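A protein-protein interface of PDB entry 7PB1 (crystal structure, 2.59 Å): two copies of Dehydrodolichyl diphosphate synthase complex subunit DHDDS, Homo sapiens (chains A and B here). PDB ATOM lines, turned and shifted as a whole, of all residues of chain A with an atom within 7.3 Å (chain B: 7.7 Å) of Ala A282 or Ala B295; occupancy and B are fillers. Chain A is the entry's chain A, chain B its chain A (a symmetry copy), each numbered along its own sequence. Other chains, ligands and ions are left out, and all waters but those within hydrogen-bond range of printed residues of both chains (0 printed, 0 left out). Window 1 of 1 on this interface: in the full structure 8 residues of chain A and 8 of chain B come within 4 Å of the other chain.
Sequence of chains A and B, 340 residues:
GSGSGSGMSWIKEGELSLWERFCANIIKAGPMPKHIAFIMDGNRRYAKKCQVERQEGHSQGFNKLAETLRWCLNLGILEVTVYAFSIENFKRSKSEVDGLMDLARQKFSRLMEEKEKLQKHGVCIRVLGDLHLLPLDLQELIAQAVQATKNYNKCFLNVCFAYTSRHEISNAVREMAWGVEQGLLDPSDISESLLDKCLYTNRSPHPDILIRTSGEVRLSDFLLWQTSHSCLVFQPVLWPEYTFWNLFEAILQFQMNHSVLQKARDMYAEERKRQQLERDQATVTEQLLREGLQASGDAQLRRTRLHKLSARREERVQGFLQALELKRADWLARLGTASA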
ATOM      1  N   GLN A 275     -20.075  26.893  -9.283  1.00  0.00           N
ATOM      2  CA  GLN A 275     -19.282  27.876  -8.549  1.00  0.00           C
ATOM      3  C   GLN A 275     -20.173  28.913  -7.877  1.00  0.00           C
ATOM      4  O   GLN A 275     -19.857  29.389  -6.781  1.00  0.00           O
ATOM      5  CB  GLN A 275     -18.285  28.558  -9.486  1.00  0.00           C
ATOM      6  CG  GLN A 275     -17.144  27.669  -9.963  1.00  0.00           C
ATOM      7  CD  GLN A 275     -16.033  28.455 -10.638  1.00  0.00           C
ATOM      8  OE1 GLN A 275     -15.682  29.552 -10.202  1.00  0.00           O
ATOM      9  NE2 GLN A 275     -15.480  27.899 -11.717  1.00  0.00           N
ATOM     10  N   GLN A 276     -21.275  29.294  -8.526  1.00  0.00           N
ATOM     11  CA  GLN A 276     -22.225  30.209  -7.905  1.00  0.00           C
ATOM     12  C   GLN A 276     -22.684  29.674  -6.560  1.00  0.00           C
ATOM     13  O   GLN A 276     -22.595  30.361  -5.537  1.00  0.00           O
ATOM     14  CB  GLN A 276     -23.427  30.425  -8.824  1.00  0.00           C
ATOM     15  CG  GLN A 276     -24.572  31.169  -8.167  1.00  0.00           C
ATOM     16  CD  GLN A 276     -24.210  32.598  -7.833  1.00  0.00           C
ATOM     17  OE1 GLN A 276     -23.741  32.893  -6.730  1.00  0.00           O
ATOM     18  NE2 GLN A 276     -24.419  33.498  -8.788  1.00  0.00           N
ATOM     19  N   LEU A 277     -23.176  28.435  -6.549  1.00  0.00           N
ATOM     20  CA  LEU A 277     -23.557  27.801  -5.295  1.00  0.00           C
ATOM     21  C   LEU A 277     -22.366  27.713  -4.354  1.00  0.00           C
ATOM     22  O   LEU A 277     -22.466  28.075  -3.176  1.00  0.00           O
ATOM     23  CB  LEU A 277     -24.137  26.415  -5.571  1.00  0.00           C
ATOM     24  CG  LEU A 277     -24.799  25.674  -4.405  1.00  0.00           C
ATOM     25  CD1 LEU A 277     -25.441  26.628  -3.407  1.00  0.00           C
ATOM     26  CD2 LEU A 277     -25.830  24.687  -4.931  1.00  0.00           C
ATOM     27  N   GLU A 278     -21.224  27.247  -4.864  1.00  0.00           N
ATOM     28  CA  GLU A 278     -20.027  27.137  -4.035  1.00  0.00           C
ATOM     29  C   GLU A 278     -19.674  28.477  -3.404  1.00  0.00           C
ATOM     30  O   GLU A 278     -19.368  28.546  -2.208  1.00  0.00           O
ATOM     31  CB  GLU A 278     -18.857  26.600  -4.865  1.00  0.00           C
ATOM     32  N   ARG A 279     -19.730  29.559  -4.184  1.00  0.00           N
ATOM     33  CA  ARG A 279     -19.465  30.878  -3.622  1.00  0.00           C
ATOM     34  C   ARG A 279     -20.613  31.351  -2.740  1.00  0.00           C
ATOM     35  O   ARG A 279     -20.391  32.089  -1.774  1.00  0.00           O
ATOM     36  CB  ARG A 279     -19.204  31.890  -4.740  1.00  0.00           C
ATOM     37  N   ASP A 280     -21.842  30.935  -3.049  1.00  0.00           N
ATOM     38  CA  ASP A 280     -22.984  31.375  -2.258  1.00  0.00           C
ATOM     39  C   ASP A 280     -22.964  30.748  -0.870  1.00  0.00           C
ATOM     40  O   ASP A 280     -23.023  31.457   0.142  1.00  0.00           O
ATOM     41  CB  ASP A 280     -24.288  31.043  -2.988  1.00  0.00           C
ATOM     42  N   GLN A 281     -22.862  29.419  -0.799  1.00  0.00           N
ATOM     43  CA  GLN A 281     -22.913  28.746   0.494  1.00  0.00           C
ATOM     44  C   GLN A 281     -21.739  29.115   1.390  1.00  0.00           C
ATOM     45  O   GLN A 281     -21.819  28.923   2.607  1.00  0.00           O
ATOM     46  CB  GLN A 281     -22.972  27.235   0.290  1.00  0.00           C
ATOM     47  CG  GLN A 281     -24.388  26.699   0.212  1.00  0.00           C
ATOM     48  CD  GLN A 281     -24.451  25.283  -0.318  1.00  0.00           C
ATOM     49  OE1 GLN A 281     -23.518  24.806  -0.967  1.00  0.00           O
ATOM     50  NE2 GLN A 281     -25.558  24.599  -0.045  1.00  0.00           N
ATOM     51  N   ALA A 282     -20.655  29.646   0.819  1.00  0.00           N
ATOM     52  CA  ALA A 282     -19.546  30.118   1.638  1.00  0.00           C
ATOM     53  C   ALA A 282     -19.981  31.271   2.529  1.00  0.00           C
ATOM     54  O   ALA A 282     -19.698  31.282   3.734  1.00  0.00           O
ATOM     55  CB  ALA A 282     -18.376  30.539   0.751  1.00  0.00           C
ATOM     56  N   THR A 283     -20.682  32.255   1.955  1.00  0.00           N
ATOM     57  CA  THR A 283     -21.104  33.406   2.750  1.00  0.00           C
ATOM     58  C   THR A 283     -22.163  33.015   3.773  1.00  0.00           C
ATOM     59  O   THR A 283     -22.146  33.508   4.910  1.00  0.00           O
ATOM     60  CB  THR A 283     -21.621  34.522   1.845  1.00  0.00           C
ATOM     61  OG1 THR A 283     -22.350  33.951   0.755  1.00  0.00           O
ATOM     62  CG2 THR A 283     -20.462  35.354   1.305  1.00  0.00           C
ATOM     63  N   VAL A 284     -23.091  32.131   3.393  1.00  0.00           N
ATOM     64  CA  VAL A 284     -24.064  31.633   4.360  1.00  0.00           C
ATOM     65  C   VAL A 284     -23.356  30.895   5.483  1.00  0.00           C
ATOM     66  O   VAL A 284     -23.787  30.950   6.641  1.00  0.00           O
ATOM     67  CB  VAL A 284     -25.114  30.743   3.669  1.00  0.00           C
ATOM     68  N   THR A 285     -22.255  30.208   5.177  1.00  0.00           N
ATOM     69  CA  THR A 285     -21.429  29.663   6.249  1.00  0.00           C
ATOM     70  C   THR A 285     -20.821  30.788   7.078  1.00  0.00           C
ATOM     71  O   THR A 285     -20.834  30.734   8.313  1.00  0.00           O
ATOM     72  CB  THR A 285     -20.337  28.753   5.677  1.00  0.00           C
ATOM     73  N   GLU A 286     -20.319  31.836   6.416  1.00  0.00           N
ATOM     74  CA  GLU A 286     -19.721  32.954   7.141  1.00  0.00           C
ATOM     75  C   GLU A 286     -20.732  33.621   8.066  1.00  0.00           C
ATOM     76  O   GLU A 286     -20.421  33.921   9.225  1.00  0.00           O
ATOM     77  CB  GLU A 286     -19.145  33.972   6.156  1.00  0.00           C
ATOM     78  N   GLN A 287     -21.953  33.853   7.574  1.00  0.00           N
ATOM     79  CA  GLN A 287     -22.969  34.504   8.396  1.00  0.00           C
ATOM     80  C   GLN A 287     -23.326  33.655   9.608  1.00  0.00           C
ATOM     81  O   GLN A 287     -23.441  34.171  10.726  1.00  0.00           O
ATOM     82  CB  GLN A 287     -24.213  34.798   7.558  1.00  0.00           C
ATOM     83  N   LEU A 288     -23.499  32.345   9.408  1.00  0.00           N
ATOM     84  CA  LEU A 288     -23.811  31.461  10.528  1.00  0.00           C
ATOM     85  C   LEU A 288     -22.652  31.385  11.511  1.00  0.00           C
ATOM     86  O   LEU A 288     -22.869  31.302  12.726  1.00  0.00           O
ATOM     87  CB  LEU A 288     -24.165  30.066  10.016  1.00  0.00           C
ATOM     88  CG  LEU A 288     -25.515  29.940   9.314  1.00  0.00           C
ATOM     89  CD1 LEU A 288     -25.873  28.480   9.087  1.00  0.00           C
ATOM     90  CD2 LEU A 288     -26.589  30.639  10.132  1.00  0.00           C
ATOM     91  N   GLN B 281     -18.396  21.097   4.308  1.00  0.00           N
ATOM     92  CA  GLN B 281     -18.011  22.233   3.477  1.00  0.00           C
ATOM     93  C   GLN B 281     -17.976  23.540   4.256  1.00  0.00           C
ATOM     94  O   GLN B 281     -17.343  24.500   3.805  1.00  0.00           O
ATOM     95  CB  GLN B 281     -18.959  22.347   2.286  1.00  0.00           C
ATOM     96  CG  GLN B 281     -18.479  21.584   1.068  1.00  0.00           C
ATOM     97  CD  GLN B 281     -19.556  21.418   0.018  1.00  0.00           C
ATOM     98  OE1 GLN B 281     -20.749  21.536   0.308  1.00  0.00           O
ATOM     99  NE2 GLN B 281     -19.143  21.142  -1.215  1.00  0.00           N
ATOM    100  N   ALA B 282     -18.635  23.599   5.415  1.00  0.00           N
ATOM    101  CA  ALA B 282     -18.547  24.788   6.254  1.00  0.00           C
ATOM    102  C   ALA B 282     -17.121  25.008   6.736  1.00  0.00           C
ATOM    103  O   ALA B 282     -16.592  26.124   6.656  1.00  0.00           O
ATOM    104  CB  ALA B 282     -19.500  24.668   7.442  1.00  0.00           C
ATOM    105  N   VAL B 284     -14.309  23.735   5.460  1.00  0.00           N
ATOM    106  CA  VAL B 284     -13.470  24.048   4.307  1.00  0.00           C
ATOM    107  C   VAL B 284     -13.666  25.496   3.894  1.00  0.00           C
ATOM    108  O   VAL B 284     -12.719  26.156   3.450  1.00  0.00           O
ATOM    109  CB  VAL B 284     -13.759  23.081   3.144  1.00  0.00           C
ATOM    110  N   THR B 285     -14.881  26.025   4.042  1.00  0.00           N
ATOM    111  CA  THR B 285     -15.065  27.461   3.860  1.00  0.00           C
ATOM    112  C   THR B 285     -14.303  28.236   4.928  1.00  0.00           C
ATOM    113  O   THR B 285     -13.620  29.220   4.622  1.00  0.00           O
ATOM    114  CB  THR B 285     -16.554  27.819   3.880  1.00  0.00           C
ATOM    115  N   GLU B 286     -14.376  27.783   6.184  1.00  0.00           N
ATOM    116  CA  GLU B 286     -13.672  28.471   7.263  1.00  0.00           C
ATOM    117  C   GLU B 286     -12.168  28.489   7.022  1.00  0.00           C
ATOM    118  O   GLU B 286     -11.515  29.525   7.198  1.00  0.00           O
ATOM    119  CB  GLU B 286     -13.990  27.810   8.605  1.00  0.00           C
ATOM    120  N   LEU B 288     -10.506  28.231   4.148  1.00  0.00           N
ATOM    121  CA  LEU B 288     -10.189  29.122   3.035  1.00  0.00           C
ATOM    122  C   LEU B 288     -10.350  30.582   3.434  1.00  0.00           C
ATOM    123  O   LEU B 288      -9.575  31.439   2.993  1.00  0.00           O
ATOM    124  CB  LEU B 288     -11.073  28.800   1.832  1.00  0.00           C
ATOM    125  CG  LEU B 288     -10.754  27.496   1.105  1.00  0.00           C
ATOM    126  CD1 LEU B 288     -11.510  27.410  -0.211  1.00  0.00           C
ATOM    127  CD2 LEU B 288      -9.255  27.386   0.877  1.00  0.00           C
ATOM    128  N   LEU B 289     -11.358  30.884   4.260  1.00  0.00           N
ATOM    129  CA  LEU B 289     -11.545  32.251   4.736  1.00  0.00           C
ATOM    130  C   LEU B 289     -10.380  32.693   5.612  1.00  0.00           C
ATOM    131  O   LEU B 289      -9.898  33.826   5.488  1.00  0.00           O
ATOM    132  CB  LEU B 289     -12.869  32.368   5.495  1.00  0.00           C
ATOM    133  N   GLY B 292      -7.677  33.083   3.490  1.00  0.00           N
ATOM    134  CA  GLY B 292      -7.991  34.191   2.607  1.00  0.00           C
ATOM    135  C   GLY B 292      -8.085  33.829   1.146  1.00  0.00           C
ATOM    136  O   GLY B 292      -8.042  34.722   0.295  1.00  0.00           O
ATOM    137  N   LEU B 293      -8.242  32.543   0.827  1.00  0.00           N
ATOM    138  CA  LEU B 293      -8.069  32.035  -0.528  1.00  0.00           C
ATOM    139  C   LEU B 293      -9.361  32.027  -1.351  1.00  0.00           C
ATOM    140  O   LEU B 293      -9.435  31.299  -2.349  1.00  0.00           O
ATOM    141  CB  LEU B 293      -7.470  30.626  -0.479  1.00  0.00           C
ATOM    142  N   GLN B 294     -10.367  32.818  -0.962  1.00  0.00           N
ATOM    143  CA  GLN B 294     -11.646  32.899  -1.669  1.00  0.00           C
ATOM    144  C   GLN B 294     -12.438  31.599  -1.578  1.00  0.00           C
ATOM    145  O   GLN B 294     -11.864  30.512  -1.461  1.00  0.00           O
ATOM    146  CB  GLN B 294     -11.438  33.277  -3.138  1.00  0.00           C
ATOM    147  CG  GLN B 294     -12.441  34.270  -3.674  1.00  0.00           C
ATOM    148  CD  GLN B 294     -12.181  34.614  -5.125  1.00  0.00           C
ATOM    149  OE1 GLN B 294     -11.827  35.746  -5.451  1.00  0.00           O
ATOM    150  NE2 GLN B 294     -12.354  33.635  -6.007  1.00  0.00           N
ATOM    151  N   ALA B 295     -13.765  31.703  -1.645  1.00  0.00           N
ATOM    152  CA  ALA B 295     -14.627  30.539  -1.474  1.00  0.00           C
ATOM    153  C   ALA B 295     -14.576  29.615  -2.687  1.00  0.00           C
ATOM    154  O   ALA B 295     -14.026  28.511  -2.609  1.00  0.00           O
ATOM    155  CB  ALA B 295     -16.068  30.978  -1.205  1.00  0.00           C
ATOM    156  N   SER B 296     -15.148  30.052  -3.807  1.00  0.00           N
ATOM    157  CA  SER B 296     -15.212  29.253  -5.020  1.00  0.00           C
ATOM    158  C   SER B 296     -14.294  29.833  -6.089  1.00  0.00           C
ATOM    159  O   SER B 296     -14.078  31.047  -6.163  1.00  0.00           O
ATOM    160  CB  SER B 296     -16.647  29.172  -5.553  1.00  0.00           C
ATOM    161  N   GLY B 297     -13.754  28.950  -6.918  1.00  0.00           N
ATOM    162  CA  GLY B 297     -12.865  29.373  -7.981  1.00  0.00           C
ATOM    163  C   GLY B 297     -12.771  28.311  -9.048  1.00  0.00           C
ATOM    164  O   GLY B 297     -13.075  27.137  -8.814  1.00  0.00           O
ATOM    165  N   GLN B 300     -10.937  25.352  -8.544  1.00  0.00           N
ATOM    166  CA  GLN B 300     -11.696  24.344  -7.804  1.00  0.00           C
ATOM    167  C   GLN B 300     -10.963  23.921  -6.535  1.00  0.00           C
ATOM    168  O   GLN B 300     -10.883  22.735  -6.206  1.00  0.00           O
ATOM    169  CB  GLN B 300     -12.013  23.133  -8.687  1.00  0.00           C
ATOM    170  CG  GLN B 300     -12.994  23.429  -9.816  1.00  0.00           C
ATOM    171  N   LEU B 301     -10.422  24.908  -5.814  1.00  0.00           N
ATOM    172  CA  LEU B 301      -9.690  24.618  -4.585  1.00  0.00           C
ATOM    173  C   LEU B 301     -10.613  24.030  -3.525  1.00  0.00           C
ATOM    174  O   LEU B 301     -10.290  23.011  -2.905  1.00  0.00           O
ATOM    175  CB  LEU B 301      -9.002  25.883  -4.067  1.00  0.00           C
ATOM    176  CG  LEU B 301      -7.773  26.358  -4.849  1.00  0.00           C
ATOM    177  N   ARG B 302     -11.773  24.659  -3.304  1.00  0.00           N
ATOM    178  CA  ARG B 302     -12.746  24.097  -2.371  1.00  0.00           C
ATOM    179  C   ARG B 302     -13.140  22.684  -2.782  1.00  0.00           C
ATOM    180  O   ARG B 302     -13.227  21.785  -1.938  1.00  0.00           O
ATOM    181  CB  ARG B 302     -13.982  24.991  -2.285  1.00  0.00           C
ATOM    182  N   ARG B 303     -13.368  22.468  -4.079  1.00  0.00           N
ATOM    183  CA  ARG B 303     -13.663  21.122  -4.559  1.00  0.00           C
ATOM    184  C   ARG B 303     -12.517  20.167  -4.240  1.00  0.00           C
ATOM    185  O   ARG B 303     -12.735  19.086  -3.677  1.00  0.00           O
ATOM    186  CB  ARG B 303     -13.952  21.156  -6.061  1.00  0.00           C
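Ala A282 touches just one residue of chain B: Ala B295.
Ala B295 touches just one residue of chain A: Ala A282.
Printed residues of chain A within 4 Å of Gly B297: Gln A275.
Printed residues of chain B within 4 Å of Arg A279: Ser B296 (3.4 Å).
Of the printed residues of chain B, Gln A275 touches Ser B296 and Gly B297.
Of the printed residues of chain B, Glu A278 touches Ser B296 (3.5 Å).
Gln B300 touches none of the printed residues of chain A.
Leu B301 touches none of the printed residues of chain A.
The nearest residue of chain A that does not touch Ala B295 is Arg A279 (4.2 Å).
Among the printed residues, merely in contact across the chains: Ala A282 with Ala B295 (3.1 Å), Gln A275 with Gly B297 (3.4 Å), Arg A279 with Ser B296 (3.4 Å), Gln A275 with Ser B296 (3.4 Å) and Glu A278 with Ser B296 (3.5 Å).
Hydrophobic or aromatic side chains of chain A that line the printed part of chain B: Ala A282.
Along chain A the printed residues that touch a printed residue of chain B span positions 275 to 282.
Along chain B the printed residues that touch a printed residue of chain A span positions 295 to 297.
Among the printed residues, no Asp or Glu carboxylate lies within 4 Å of a Lys or Arg side-chain nitrogen of the other chain.
NE2 of Gln B294 sits at hydrogen-bond distance from O of Ser B296, at 3.1 Å.
6 positions are printed for both chains.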
